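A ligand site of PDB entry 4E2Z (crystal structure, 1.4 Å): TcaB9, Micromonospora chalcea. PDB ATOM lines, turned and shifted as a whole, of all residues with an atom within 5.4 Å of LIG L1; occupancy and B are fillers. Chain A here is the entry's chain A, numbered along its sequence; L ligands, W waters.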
ATOM      1  N   ARG A  70       1.517  -1.679  -6.077  1.00  0.00           N
ATOM      2  CA  ARG A  70       0.595  -2.807  -6.232  1.00  0.00           C
ATOM      3  C   ARG A  70       0.697  -3.873  -5.141  1.00  0.00           C
ATOM      4  O   ARG A  70      -0.286  -4.464  -4.681  1.00  0.00           O
ATOM      5  CB  ARG A  70       0.701  -3.380  -7.650  1.00  0.00           C
ATOM      6  CG  ARG A  70       2.074  -4.035  -7.936  1.00  0.00           C
ATOM      7  CD  ARG A  70       2.137  -4.546  -9.377  1.00  0.00           C
ATOM      8  NE  ARG A  70       3.405  -5.181  -9.743  1.00  0.00           N
ATOM      9  CZ  ARG A  70       3.637  -5.623 -10.976  1.00  0.00           C
ATOM     10  NH1 ARG A  70       2.686  -5.536 -11.906  1.00  0.00           N
ATOM     11  NH2 ARG A  70       4.798  -6.181 -11.257  1.00  0.00           N
ATOM     12  N   PHE A  74      -2.355  -6.003  -3.218  1.00  0.00           N
ATOM     13  CA  PHE A  74      -2.666  -7.301  -3.806  1.00  0.00           C
ATOM     14  C   PHE A  74      -1.547  -8.276  -3.458  1.00  0.00           C
ATOM     15  O   PHE A  74      -0.398  -8.043  -3.847  1.00  0.00           O
ATOM     16  CB  PHE A  74      -2.872  -7.156  -5.312  1.00  0.00           C
ATOM     17  CG  PHE A  74      -3.856  -6.058  -5.671  1.00  0.00           C
ATOM     18  CD1 PHE A  74      -5.188  -6.113  -5.298  1.00  0.00           C
ATOM     19  CD2 PHE A  74      -3.373  -4.972  -6.389  1.00  0.00           C
ATOM     20  CE1 PHE A  74      -6.087  -5.071  -5.627  1.00  0.00           C
ATOM     21  CE2 PHE A  74      -4.246  -3.926  -6.766  1.00  0.00           C
ATOM     22  CZ  PHE A  74      -5.607  -4.005  -6.391  1.00  0.00           C
ATOM     23  N   TYR A  78      -5.069 -10.770   0.451  1.00  0.00           N
ATOM     24  CA  TYR A  78      -6.150  -9.932  -0.044  1.00  0.00           C
ATOM     25  C   TYR A  78      -7.516 -10.563   0.270  1.00  0.00           C
ATOM     26  O   TYR A  78      -7.758 -11.727  -0.026  1.00  0.00           O
ATOM     27  CB  TYR A  78      -6.009  -9.786  -1.549  1.00  0.00           C
ATOM     28  CG  TYR A  78      -6.991  -8.833  -2.204  1.00  0.00           C
ATOM     29  CD1 TYR A  78      -7.985  -9.350  -3.024  1.00  0.00           C
ATOM     30  CD2 TYR A  78      -6.887  -7.456  -1.994  1.00  0.00           C
ATOM     31  CE1 TYR A  78      -8.861  -8.456  -3.658  1.00  0.00           C
ATOM     32  CE2 TYR A  78      -7.789  -6.571  -2.602  1.00  0.00           C
ATOM     33  CZ  TYR A  78      -8.760  -7.118  -3.416  1.00  0.00           C
ATOM     34  OH  TYR A  78      -9.630  -6.267  -4.057  1.00  0.00           O
ATOM     35  N   TYR A  80     -10.960  -9.843  -0.596  1.00  0.00           N
ATOM     36  CA  TYR A  80     -12.269  -9.715  -1.283  1.00  0.00           C
ATOM     37  C   TYR A  80     -12.574 -11.046  -1.970  1.00  0.00           C
ATOM     38  O   TYR A  80     -11.786 -11.548  -2.767  1.00  0.00           O
ATOM     39  CB  TYR A  80     -12.277  -8.613  -2.335  1.00  0.00           C
ATOM     40  CG  TYR A  80     -13.644  -8.464  -2.994  1.00  0.00           C
ATOM     41  CD1 TYR A  80     -14.759  -8.013  -2.277  1.00  0.00           C
ATOM     42  CD2 TYR A  80     -13.794  -8.711  -4.367  1.00  0.00           C
ATOM     43  CE1 TYR A  80     -16.023  -7.825  -2.874  1.00  0.00           C
ATOM     44  CE2 TYR A  80     -15.032  -8.574  -4.961  1.00  0.00           C
ATOM     45  CZ  TYR A  80     -16.110  -8.132  -4.211  1.00  0.00           C
ATOM     46  OH  TYR A  80     -17.335  -7.923  -4.809  1.00  0.00           O
ATOM     47  N   SER A  82     -15.161 -12.489  -4.629  1.00  0.00           N
ATOM     48  CA  SER A  82     -16.232 -12.189  -5.581  1.00  0.00           C
ATOM     49  C   SER A  82     -17.503 -12.998  -5.364  1.00  0.00           C
ATOM     50  O   SER A  82     -18.603 -12.425  -5.535  1.00  0.00           O
ATOM     51  CB  SER A  82     -15.683 -12.395  -6.995  1.00  0.00           C
ATOM     52  OG  SER A  82     -14.578 -11.505  -7.154  1.00  0.00           O
ATOM     53  N   PHE A  92     -21.812 -13.001 -13.745  1.00  0.00           N
ATOM     54  CA  PHE A  92     -20.643 -13.507 -14.436  1.00  0.00           C
ATOM     55  C   PHE A  92     -20.867 -14.854 -15.157  1.00  0.00           C
ATOM     56  O   PHE A  92     -20.286 -15.032 -16.232  1.00  0.00           O
ATOM     57  CB  PHE A  92     -19.434 -13.604 -13.477  1.00  0.00           C
ATOM     58  CG  PHE A  92     -18.852 -12.247 -13.081  1.00  0.00           C
ATOM     59  CD1 PHE A  92     -18.311 -11.383 -14.022  1.00  0.00           C
ATOM     60  CD2 PHE A  92     -18.879 -11.839 -11.748  1.00  0.00           C
ATOM     61  CE1 PHE A  92     -17.802 -10.130 -13.676  1.00  0.00           C
ATOM     62  CE2 PHE A  92     -18.350 -10.587 -11.379  1.00  0.00           C
ATOM     63  CZ  PHE A  92     -17.805  -9.748 -12.356  1.00  0.00           C
ATOM     64  N   GLU A 113      -8.539 -14.377 -18.288  1.00  0.00           N
ATOM     65  CA  GLU A 113      -9.164 -13.360 -17.428  1.00  0.00           C
ATOM     66  C   GLU A 113      -8.082 -12.721 -16.561  1.00  0.00           C
ATOM     67  O   GLU A 113      -7.263 -13.408 -15.954  1.00  0.00           O
ATOM     68  CB  GLU A 113     -10.242 -13.968 -16.510  1.00  0.00           C
ATOM     69  CG  GLU A 113     -10.926 -12.883 -15.725  1.00  0.00           C
ATOM     70  CD  GLU A 113     -12.096 -13.368 -14.886  1.00  0.00           C
ATOM     71  OE1 GLU A 113     -12.855 -12.474 -14.416  1.00  0.00           O
ATOM     72  OE2 GLU A 113     -12.241 -14.601 -14.660  1.00  0.00           O
ATOM     73  N   ILE A 114      -8.106 -11.385 -16.550  1.00  0.00           N
ATOM     74  CA  ILE A 114      -7.231 -10.579 -15.706  1.00  0.00           C
ATOM     75  C   ILE A 114      -7.957 -10.318 -14.385  1.00  0.00           C
ATOM     76  O   ILE A 114      -9.044  -9.710 -14.403  1.00  0.00           O
ATOM     77  CB  ILE A 114      -6.884  -9.227 -16.418  1.00  0.00           C
ATOM     78  CG1 ILE A 114      -6.148  -9.491 -17.739  1.00  0.00           C
ATOM     79  CG2 ILE A 114      -6.027  -8.390 -15.457  1.00  0.00           C
ATOM     80  CD1 ILE A 114      -5.867  -8.202 -18.554  1.00  0.00           C
ATOM     81  N   GLY A 115      -7.491 -10.799 -13.245  1.00  0.00           N
ATOM     82  CA  GLY A 115      -8.227 -10.580 -12.005  1.00  0.00           C
ATOM     83  C   GLY A 115      -9.323 -11.592 -11.746  1.00  0.00           C
ATOM     84  O   GLY A 115     -10.418 -11.190 -11.304  1.00  0.00           O
ATOM     85  N   CYS A 116      -9.079 -12.896 -11.950  1.00  0.00           N
ATOM     86  CA  CYS A 116     -10.163 -13.865 -11.846  1.00  0.00           C
ATOM     87  C   CYS A 116     -10.700 -14.112 -10.440  1.00  0.00           C
ATOM     88  O   CYS A 116     -11.750 -14.733 -10.261  1.00  0.00           O
ATOM     89  CB  CYS A 116      -9.793 -15.213 -12.475  1.00  0.00           C
ATOM     90  SG  CYS A 116      -8.435 -16.119 -11.693  1.00  0.00           S
ATOM     91  N   ASN A 117      -9.977 -13.681  -9.402  1.00  0.00           N
ATOM     92  CA  ASN A 117     -10.379 -13.806  -8.007  1.00  0.00           C
ATOM     93  C   ASN A 117     -10.674 -15.265  -7.722  1.00  0.00           C
ATOM     94  O   ASN A 117      -9.930 -16.133  -8.146  1.00  0.00           O
ATOM     95  CB  ASN A 117     -11.510 -12.788  -7.711  1.00  0.00           C
ATOM     96  CG  ASN A 117     -11.717 -12.619  -6.223  1.00  0.00           C
ATOM     97  OD1 ASN A 117     -12.555 -13.285  -5.596  1.00  0.00           O
ATOM     98  ND2 ASN A 117     -10.937 -11.725  -5.629  1.00  0.00           N
ATOM     99  N   ILE A 120     -15.187 -16.812 -10.028  1.00  0.00           N
ATOM    100  CA  ILE A 120     -16.595 -16.463 -10.302  1.00  0.00           C
ATOM    101  C   ILE A 120     -17.069 -16.556 -11.765  1.00  0.00           C
ATOM    102  O   ILE A 120     -18.191 -16.994 -12.082  1.00  0.00           O
ATOM    103  CB  ILE A 120     -16.956 -15.082  -9.645  1.00  0.00           C
ATOM    104  CG1 ILE A 120     -18.474 -14.829  -9.643  1.00  0.00           C
ATOM    105  CG2 ILE A 120     -16.151 -13.932 -10.281  1.00  0.00           C
ATOM    106  CD1 ILE A 120     -18.857 -13.752  -8.629  1.00  0.00           C
ATOM    107  N   PHE A 135      -5.349 -14.814 -14.426  1.00  0.00           N
ATOM    108  CA  PHE A 135      -4.223 -14.139 -13.763  1.00  0.00           C
ATOM    109  C   PHE A 135      -4.782 -13.679 -12.412  1.00  0.00           C
ATOM    110  O   PHE A 135      -5.799 -12.972 -12.350  1.00  0.00           O
ATOM    111  CB  PHE A 135      -3.731 -12.904 -14.532  1.00  0.00           C
ATOM    112  CG  PHE A 135      -2.763 -13.253 -15.616  1.00  0.00           C
ATOM    113  CD1 PHE A 135      -1.402 -13.137 -15.387  1.00  0.00           C
ATOM    114  CD2 PHE A 135      -3.201 -13.688 -16.867  1.00  0.00           C
ATOM    115  CE1 PHE A 135      -0.488 -13.444 -16.397  1.00  0.00           C
ATOM    116  CE2 PHE A 135      -2.294 -14.022 -17.893  1.00  0.00           C
ATOM    117  CZ  PHE A 135      -0.930 -13.891 -17.640  1.00  0.00           C
ATOM    118  N   GLU A 136      -4.158 -14.069 -11.316  1.00  0.00           N
ATOM    119  CA  GLU A 136      -4.665 -13.715  -9.991  1.00  0.00           C
ATOM    120  C   GLU A 136      -3.416 -13.603  -9.108  1.00  0.00           C
ATOM    121  O   GLU A 136      -2.973 -14.656  -8.600  1.00  0.00           O
ATOM    122  CB  GLU A 136      -5.753 -14.690  -9.497  1.00  0.00           C
ATOM    123  CG  GLU A 136      -6.454 -14.259  -8.200  1.00  0.00           C
ATOM    124  CD  GLU A 136      -6.551 -12.746  -8.121  1.00  0.00           C
ATOM    125  OE1 GLU A 136      -7.540 -12.216  -8.657  1.00  0.00           O
ATOM    126  OE2 GLU A 136      -5.637 -12.069  -7.596  1.00  0.00           O
ATOM    127  N   PRO A 137      -2.906 -12.371  -8.900  1.00  0.00           N
ATOM    128  CA  PRO A 137      -1.661 -12.227  -8.145  1.00  0.00           C
ATOM    129  C   PRO A 137      -1.897 -12.342  -6.645  1.00  0.00           C
ATOM    130  O   PRO A 137      -0.905 -12.300  -5.901  1.00  0.00           O
ATOM    131  CB  PRO A 137      -1.251 -10.781  -8.481  1.00  0.00           C
ATOM    132  CG  PRO A 137      -2.573 -10.035  -8.777  1.00  0.00           C
ATOM    133  CD  PRO A 137      -3.283 -11.107  -9.573  1.00  0.00           C
ATOM    134  N   SER A 138      -3.155 -12.417  -6.196  1.00  0.00           N
ATOM    135  CA  SER A 138      -3.504 -12.571  -4.790  1.00  0.00           C
ATOM    136  C   SER A 138      -3.693 -14.071  -4.561  1.00  0.00           C
ATOM    137  O   SER A 138      -4.697 -14.672  -4.928  1.00  0.00           O
ATOM    138  CB  SER A 138      -4.715 -11.719  -4.373  1.00  0.00           C
ATOM    139  OG  SER A 138      -4.452 -10.322  -4.449  1.00  0.00           O
ATOM    140  N   VAL A 141      -7.014 -16.057  -2.847  1.00  0.00           N
ATOM    141  CA  VAL A 141      -8.199 -16.195  -3.707  1.00  0.00           C
ATOM    142  C   VAL A 141      -7.884 -17.035  -4.949  1.00  0.00           C
ATOM    143  O   VAL A 141      -8.751 -17.785  -5.411  1.00  0.00           O
ATOM    144  CB  VAL A 141      -8.869 -14.825  -3.993  1.00  0.00           C
ATOM    145  CG1 VAL A 141      -9.404 -14.145  -2.739  1.00  0.00           C
ATOM    146  CG2 VAL A 141      -7.900 -13.898  -4.716  1.00  0.00           C
ATOM    147  N   ASP A 155       0.183 -14.241 -10.755  1.00  0.00           N
ATOM    148  CA  ASP A 155       1.081 -13.208 -11.290  1.00  0.00           C
ATOM    149  C   ASP A 155       0.200 -12.022 -11.660  1.00  0.00           C
ATOM    150  O   ASP A 155      -0.971 -12.247 -11.949  1.00  0.00           O
ATOM    151  CB  ASP A 155       1.702 -13.637 -12.627  1.00  0.00           C
ATOM    152  CG  ASP A 155       3.029 -14.360 -12.480  1.00  0.00           C
ATOM    153  OD1 ASP A 155       3.145 -15.496 -12.994  1.00  0.00           O
ATOM    154  OD2 ASP A 155       3.941 -13.770 -11.860  1.00  0.00           O
ATOM    155  N   PHE A 156       0.741 -10.809 -11.729  1.00  0.00           N
ATOM    156  CA  PHE A 156       0.040  -9.646 -12.276  1.00  0.00           C
ATOM    157  C   PHE A 156       0.123  -9.813 -13.790  1.00  0.00           C
ATOM    158  O   PHE A 156       1.153 -10.149 -14.381  1.00  0.00           O
ATOM    159  CB  PHE A 156       0.898  -8.419 -11.914  1.00  0.00           C
ATOM    160  CG  PHE A 156       0.878  -8.125 -10.429  1.00  0.00           C
ATOM    161  CD1 PHE A 156      -0.276  -7.503  -9.929  1.00  0.00           C
ATOM    162  CD2 PHE A 156       1.927  -8.409  -9.559  1.00  0.00           C
ATOM    163  CE1 PHE A 156      -0.382  -7.206  -8.566  1.00  0.00           C
ATOM    164  CE2 PHE A 156       1.835  -8.130  -8.188  1.00  0.00           C
ATOM    165  CZ  PHE A 156       0.692  -7.476  -7.700  1.00  0.00           C
ATOM    166  N   PHE A 157      -0.982  -9.543 -14.485  1.00  0.00           N
ATOM    167  CA  PHE A 157      -0.937  -9.258 -15.912  1.00  0.00           C
ATOM    168  C   PHE A 157      -0.197  -7.955 -16.206  1.00  0.00           C
ATOM    169  O   PHE A 157      -0.506  -6.916 -15.622  1.00  0.00           O
ATOM    170  CB  PHE A 157      -2.368  -9.325 -16.478  1.00  0.00           C
ATOM    171  CG  PHE A 157      -2.442  -9.327 -17.988  1.00  0.00           C
ATOM    172  CD1 PHE A 157      -2.274  -8.139 -18.682  1.00  0.00           C
ATOM    173  CD2 PHE A 157      -2.679 -10.509 -18.667  1.00  0.00           C
ATOM    174  CE1 PHE A 157      -2.360  -8.122 -20.076  1.00  0.00           C
ATOM    175  CE2 PHE A 157      -2.721 -10.491 -20.076  1.00  0.00           C
ATOM    176  CZ  PHE A 157      -2.598  -9.311 -20.767  1.00  0.00           C
ATOM    177  N   GLU A 158       0.737  -8.026 -17.155  1.00  0.00           N
ATOM    178  CA  GLU A 158       1.510  -6.883 -17.632  1.00  0.00           C
ATOM    179  C   GLU A 158       2.202  -7.404 -18.897  1.00  0.00           C
ATOM    180  O   GLU A 158       2.061  -8.589 -19.236  1.00  0.00           O
ATOM    181  CB  GLU A 158       2.555  -6.398 -16.606  1.00  0.00           C
ATOM    182  CG  GLU A 158       3.512  -7.462 -16.131  1.00  0.00           C
ATOM    183  CD  GLU A 158       4.553  -6.994 -15.119  1.00  0.00           C
ATOM    184  OE1 GLU A 158       5.725  -6.708 -15.444  1.00  0.00           O
ATOM    185  OE2 GLU A 158       4.207  -6.947 -13.929  1.00  0.00           O
ATOM    186  N   ALA A 178     -12.808  -7.665 -15.101  1.00  0.00           N
ATOM    187  CA  ALA A 178     -13.932  -6.959 -14.457  1.00  0.00           C
ATOM    188  C   ALA A 178     -13.474  -6.353 -13.139  1.00  0.00           C
ATOM    189  O   ALA A 178     -12.883  -7.060 -12.337  1.00  0.00           O
ATOM    190  CB  ALA A 178     -15.098  -7.917 -14.155  1.00  0.00           C
ATOM    191  N   ASN A 179     -13.732  -5.052 -12.906  1.00  0.00           N
ATOM    192  CA  ASN A 179     -13.314  -4.447 -11.624  1.00  0.00           C
ATOM    193  C   ASN A 179     -11.819  -4.584 -11.317  1.00  0.00           C
ATOM    194  O   ASN A 179     -11.460  -4.673 -10.151  1.00  0.00           O
ATOM    195  CB  ASN A 179     -14.206  -4.962 -10.479  1.00  0.00           C
ATOM    196  CG  ASN A 179     -15.670  -4.801 -10.839  1.00  0.00           C
ATOM    197  OD1 ASN A 179     -16.093  -3.670 -11.072  1.00  0.00           O
ATOM    198  ND2 ASN A 179     -16.413  -5.921 -10.940  1.00  0.00           N
ATOM    199  N   THR A 180     -11.041  -4.609 -12.389  1.00  0.00           N
ATOM    200  CA  THR A 180      -9.600  -4.847 -12.263  1.00  0.00           C
ATOM    201  C   THR A 180      -8.784  -3.821 -13.066  1.00  0.00           C
ATOM    202  O   THR A 180      -7.805  -3.214 -12.599  1.00  0.00           O
ATOM    203  CB  THR A 180      -9.275  -6.306 -12.725  1.00  0.00           C
ATOM    204  OG1 THR A 180      -9.990  -7.205 -11.863  1.00  0.00           O
ATOM    205  CG2 THR A 180      -7.802  -6.613 -12.619  1.00  0.00           C
ATOM    206  N   HIS A 183      -7.915  -0.483 -11.494  1.00  0.00           N
ATOM    207  CA  HIS A 183      -6.896  -0.273 -10.455  1.00  0.00           C
ATOM    208  C   HIS A 183      -5.462  -0.474 -10.919  1.00  0.00           C
ATOM    209  O   HIS A 183      -4.584  -0.605 -10.069  1.00  0.00           O
ATOM    210  CB  HIS A 183      -7.218  -0.875  -9.096  1.00  0.00           C
ATOM    211  CG  HIS A 183      -7.458  -2.345  -9.104  1.00  0.00           C
ATOM    212  ND1 HIS A 183      -8.630  -2.901  -8.639  1.00  0.00           N
ATOM    213  CD2 HIS A 183      -6.637  -3.381  -9.420  1.00  0.00           C
ATOM    214  CE1 HIS A 183      -8.525  -4.226  -8.709  1.00  0.00           C
ATOM    215  NE2 HIS A 183      -7.337  -4.539  -9.195  1.00  0.00           N
ATOM    216  N   ILE A 184      -5.244  -0.515 -12.237  1.00  0.00           N
ATOM    217  CA  ILE A 184      -3.892  -0.747 -12.737  1.00  0.00           C
ATOM    218  C   ILE A 184      -3.376   0.558 -13.335  1.00  0.00           C
ATOM    219  O   ILE A 184      -3.746   0.880 -14.475  1.00  0.00           O
ATOM    220  CB  ILE A 184      -3.915  -1.913 -13.756  1.00  0.00           C
ATOM    221  CG1 ILE A 184      -4.306  -3.201 -13.027  1.00  0.00           C
ATOM    222  CG2 ILE A 184      -2.501  -2.067 -14.346  1.00  0.00           C
ATOM    223  CD1 ILE A 184      -4.521  -4.392 -13.962  1.00  0.00           C
ATOM    224  N   TYR A 186      -0.526   1.187 -14.425  1.00  0.00           N
ATOM    225  CA  TYR A 186       0.368   0.800 -15.526  1.00  0.00           C
ATOM    226  C   TYR A 186      -0.385   0.213 -16.722  1.00  0.00           C
ATOM    227  O   TYR A 186      -0.041  -0.815 -17.310  1.00  0.00           O
ATOM    228  CB  TYR A 186       1.514  -0.094 -15.014  1.00  0.00           C
ATOM    229  CG  TYR A 186       1.061  -1.298 -14.202  1.00  0.00           C
ATOM    230  CD1 TYR A 186       0.796  -1.200 -12.838  1.00  0.00           C
ATOM    231  CD2 TYR A 186       0.924  -2.550 -14.801  1.00  0.00           C
ATOM    232  CE1 TYR A 186       0.388  -2.307 -12.084  1.00  0.00           C
ATOM    233  CE2 TYR A 186       0.481  -3.639 -14.079  1.00  0.00           C
ATOM    234  CZ  TYR A 186       0.210  -3.527 -12.722  1.00  0.00           C
ATOM    235  OH  TYR A 186      -0.163  -4.586 -11.944  1.00  0.00           O
ATOM    236  N   VAL A 190      -0.321  -3.002 -19.605  1.00  0.00           N
ATOM    237  CA  VAL A 190      -1.395  -3.965 -19.848  1.00  0.00           C
ATOM    238  C   VAL A 190      -1.795  -3.961 -21.323  1.00  0.00           C
ATOM    239  O   VAL A 190      -1.974  -5.039 -21.881  1.00  0.00           O
ATOM    240  CB  VAL A 190      -2.625  -3.708 -18.937  1.00  0.00           C
ATOM    241  CG1 VAL A 190      -3.797  -4.584 -19.379  1.00  0.00           C
ATOM    242  CG2 VAL A 190      -2.251  -3.927 -17.477  1.00  0.00           C
ATOM    243  N   HIS A 256     -22.418  -2.845  -9.080  1.00  0.00           N
ATOM    244  CA  HIS A 256     -21.393  -1.973  -8.481  1.00  0.00           C
ATOM    245  C   HIS A 256     -21.670  -0.488  -8.543  1.00  0.00           C
ATOM    246  O   HIS A 256     -20.698   0.292  -8.658  1.00  0.00           O
ATOM    247  CB  HIS A 256     -19.984  -2.377  -8.917  1.00  0.00           C
ATOM    248  CG  HIS A 256     -19.558  -3.709  -8.385  1.00  0.00           C
ATOM    249  ND1 HIS A 256     -19.444  -3.971  -7.038  1.00  0.00           N
ATOM    250  CD2 HIS A 256     -19.253  -4.870  -9.036  1.00  0.00           C
ATOM    251  CE1 HIS A 256     -19.116  -5.248  -6.877  1.00  0.00           C
ATOM    252  NE2 HIS A 256     -18.965  -5.803  -8.070  1.00  0.00           N
HETATM  253  N1  LIG L   1     -13.031  -9.908 -11.370  1.00  0.00           N
HETATM  254  C1  LIG L   1     -13.403  -9.960  -9.915  1.00  0.00           C
HETATM  255  C2  LIG L   1     -12.194  -9.406  -9.164  1.00  0.00           C
HETATM  256  C3  LIG L   1     -12.422  -8.196  -8.278  1.00  0.00           C
HETATM  257  S1  LIG L   1     -10.980  -8.112  -7.255  1.00  0.00           S
HETATM  258  C4  LIG L   1     -14.739  -9.282  -9.775  1.00  0.00           C
HETATM  259  O1  LIG L   1     -15.133  -8.536 -10.678  1.00  0.00           O
HETATM  260  O2  LIG L   1     -15.382  -9.436  -8.753  1.00  0.00           O
HETATM  261  C5  LIG L   1      -9.689  -7.368  -8.212  1.00  0.00           C
HETATM  262  C6  LIG L   1      -8.620  -8.441  -8.465  1.00  0.00           C
HETATM  263  O3  LIG L   1      -7.626  -7.849  -9.304  1.00  0.00           O
HETATM  264  C7  LIG L   1      -7.932  -8.889  -7.168  1.00  0.00           C
HETATM  265  O4  LIG L   1      -8.233 -10.287  -6.994  1.00  0.00           O
HETATM  266  C8  LIG L   1      -6.442  -8.656  -7.454  1.00  0.00           C
HETATM  267  O5  LIG L   1      -5.428  -9.533  -6.934  1.00  0.00           O
HETATM  268  C9  LIG L   1      -6.457  -8.639  -8.984  1.00  0.00           C
HETATM  269  N2  LIG L   1      -5.340  -7.894  -9.633  1.00  0.00           N
HETATM  270  C10 LIG L   1      -4.711  -6.729  -9.300  1.00  0.00           C
HETATM  271  N3  LIG L   1      -3.819  -6.303 -10.206  1.00  0.00           N
HETATM  272  C11 LIG L   1      -3.788  -7.261 -11.177  1.00  0.00           C
HETATM  273  C12 LIG L   1      -3.071  -7.444 -12.453  1.00  0.00           C
HETATM  274  N4  LIG L   1      -2.119  -6.582 -12.882  1.00  0.00           N
HETATM  275  N5  LIG L   1      -3.400  -8.604 -13.056  1.00  0.00           N
HETATM  276  C13 LIG L   1      -4.351  -9.509 -12.717  1.00  0.00           C
HETATM  277  N6  LIG L   1      -5.048  -9.386 -11.574  1.00  0.00           N
HETATM  278  C14 LIG L   1      -4.822  -8.259 -10.836  1.00  0.00           C
HETATM  279  P1  LG2 L   2     -18.587  -5.020  -2.595  1.00  0.00           P
HETATM  280  C1  LG2 L   2     -14.200  -4.691  -3.735  1.00  0.00           C
HETATM  281  O1  LG2 L   2     -14.903  -3.485  -3.432  1.00  0.00           O
HETATM  282  C2  LG2 L   2     -12.717  -4.407  -4.002  1.00  0.00           C
HETATM  283  P2  LG2 L   2     -15.994  -3.504  -2.263  1.00  0.00           P
HETATM  284  C3  LG2 L   2     -12.536  -4.104  -5.501  1.00  0.00           C
HETATM  285  N1  LG2 L   2     -11.462  -3.121  -5.696  1.00  0.00           N
HETATM  286  C4  LG2 L   2     -13.816  -3.767  -6.245  1.00  0.00           C
HETATM  287  O2  LG2 L   2     -13.868  -2.857  -7.064  1.00  0.00           O
HETATM  288  C5  LG2 L   2     -15.102  -4.512  -5.966  1.00  0.00           C
HETATM  289  O3  LG2 L   2     -14.823  -5.349  -4.848  1.00  0.00           O
HETATM  290  C6  LG2 L   2     -15.549  -5.446  -7.092  1.00  0.00           C
HETATM  291  C7  LG2 L   2     -20.496  -7.911   2.157  1.00  0.00           C
HETATM  292  N2  LG2 L   2     -21.805  -8.505   1.838  1.00  0.00           N
HETATM  293  O4  LG2 L   2     -18.977  -6.247  -3.425  1.00  0.00           O
HETATM  294  C8  LG2 L   2     -19.430  -8.689   1.389  1.00  0.00           C
HETATM  295  C9  LG2 L   2     -22.527  -8.970   2.869  1.00  0.00           C
HETATM  296  O5  LG2 L   2     -22.215  -8.937   4.074  1.00  0.00           O
HETATM  297  O6  LG2 L   2     -19.517  -3.859  -2.616  1.00  0.00           O
HETATM  298  C10 LG2 L   2     -18.372  -7.647   1.060  1.00  0.00           C
HETATM  299  O7  LG2 L   2     -17.360  -7.588   2.108  1.00  0.00           O
HETATM  300  N3  LG2 L   2     -23.768  -9.506   2.621  1.00  0.00           N
HETATM  301  C11 LG2 L   2     -11.972  -5.353  -6.210  1.00  0.00           C
HETATM  302  O8  LG2 L   2     -16.580  -2.130  -2.138  1.00  0.00           O
HETATM  303  C12 LG2 L   2     -19.158  -6.343   0.972  1.00  0.00           C
HETATM  304  O9  LG2 L   2     -20.367  -6.579   1.672  1.00  0.00           O
HETATM  305  C13 LG2 L   2     -24.218  -9.654   1.355  1.00  0.00           C
HETATM  306  O10 LG2 L   2     -25.362 -10.141   1.139  1.00  0.00           O
HETATM  307  O11 LG2 L   2     -15.486  -4.162  -1.020  1.00  0.00           O
HETATM  308  C14 LG2 L   2     -19.627  -5.950  -0.423  1.00  0.00           C
HETATM  309  O12 LG2 L   2     -18.447  -5.500  -1.083  1.00  0.00           O
HETATM  310  C15 LG2 L   2     -23.442  -9.104   0.214  1.00  0.00           C
HETATM  311  C16 LG2 L   2     -23.905  -9.188  -1.215  1.00  0.00           C
HETATM  312  C17 LG2 L   2     -22.208  -8.544   0.548  1.00  0.00           C
HETATM  313  O13 LG2 L   2     -17.096  -4.487  -2.883  1.00  0.00           O
HETATM  314  O   HOH W   1     -11.859  -9.949 -13.959  1.00  0.00           O
HETATM  315  O   HOH W   2     -14.815 -11.736 -12.736  1.00  0.00           O
HETATM  316  O   HOH W   3     -17.859  -8.459  -8.125  1.00  0.00           O
HETATM  317  O   HOH W   4      -1.769  -4.220  -9.886  1.00  0.00           O
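Phe 74 touches LIG L1. CE1 of Tyr 78 touches C7 of LIG L1, at 3.7 Å. Tyr 80 touches LIG L1 (CE2 to O2, 3.9 Å). Phe 92 touches LIG L1. Ile 114 touches LIG L1 (CG2 to C13, 3.4 Å). Phe 135 touches LIG L1. Pro 137 touches LIG L1 (CD to N6, 3.2 Å). Phe 156 touches LIG L1 (CD1 to N4, 3.6 Å). Thr 180 touches LIG L1. CD1 of Ile 184 touches N4 of LIG L1, 3.4 Å away. Hydrophobic or aromatic side chains within 4 Å of LIG L1: Phe 74, Tyr 78, Tyr 80, Phe 92, Ile 114, Phe 135, Pro 137, Phe 156, Phe 157, Ala 178, His 183, Ile 184 and Tyr 186. Of the 29 residues printed, 21 come within 4 Å of LIG L1. The nearest printed residue that does not touch LIG L1 is Val 141 (4.3 Å).
Water W3 lies within hydrogen-bond range of O2 of LIG L1, NE2 of His 256 and OH of Tyr 80. Water W2 lies within hydrogen-bond range of the side-chain carboxylate of Glu 113 (2.7 Å) and a nitrogen (N1) of LIG L1 (2.9 Å). Water W4 bridges OH of Tyr 186 and N3 of LIG L1.
OE2 of Glu 136 is in hydrogen-bond range of N of Ser 138. The backbone NH (N) of Asn 117 lies within hydrogen-bond range of the side-chain carboxylate (OE1) of Glu 136 (2.9 Å). The backbone NH (N) of Ser 82 sits at hydrogen-bond distance from the side-chain amide oxygen (OD1) of Asn 117 (2.9 Å). The backbone carbonyl oxygen (O) of Phe 135 is in hydrogen-bond range of the backbone NH (N) of Gly 115 (2.9 Å). The side-chain hydroxyl of Tyr 186 lies within hydrogen-bond range of the guanidinium group of Arg 70 (3.0 Å). The backbone carbonyl oxygen of Tyr 80 sits at hydrogen-bond distance from the side-chain amide nitrogen of Asn 117. O of Glu 113 is in hydrogen-bond range of N of Phe 135, at 2.8 Å. The backbone carbonyl oxygen of Phe 135 lies within hydrogen-bond range of the backbone NH of Cys 116 (3.3 Å).
An oxygen (O5) of LIG L1 lies within hydrogen-bond range of the side-chain carboxylate of Glu 136, at 2.6 Å. OG of Ser 82 is in hydrogen-bond range of O2 of LIG L1, 2.7 Å away. The side-chain hydroxyl (OG) of Ser 138 sits at hydrogen-bond distance from an oxygen (O5) of LIG L1 (2.8 Å). N of Gly 115 lies within hydrogen-bond range of N6 of LIG L1. The backbone carbonyl oxygen (O) of Gly 115 sits at hydrogen-bond distance from a nitrogen (N1) of LIG L1 (2.9 Å). ND2 of Asn 179 lies within hydrogen-bond range of O1 of LIG L1 (2.9 Å). The side-chain hydroxyl (OH) of Tyr 186 is in hydrogen-bond range of a nitrogen (N4) of LIG L1 (2.9 Å). N5 of LIG L1 lies within hydrogen-bond range of N of Phe 157 (3.0 Å). The backbone carbonyl oxygen (O) of Phe 157 lies within hydrogen-bond range of a nitrogen (N4) of LIG L1. A nitrogen (N1) of LIG L1 lies within hydrogen-bond range of the backbone carbonyl oxygen of Ala 178, 3.0 Å away. An oxygen (O3) of LIG L1 lies within hydrogen-bond range of a ring nitrogen (NE2) of His 183 (3.3 Å). The side-chain amide nitrogen (ND2) of Asn 117 lies within hydrogen-bond range of an oxygen (O4) of LIG L1 (3.4 Å). The side-chain carboxylate (OE1) of Glu 113 is in salt-bridge range of a nitrogen (N1) of LIG L1 (3.99 Å). The side-chain hydroxyl (OH) of Tyr 80 lies within hydrogen-bond range of an oxygen (O4) of LG2 L2 (2.7 Å).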
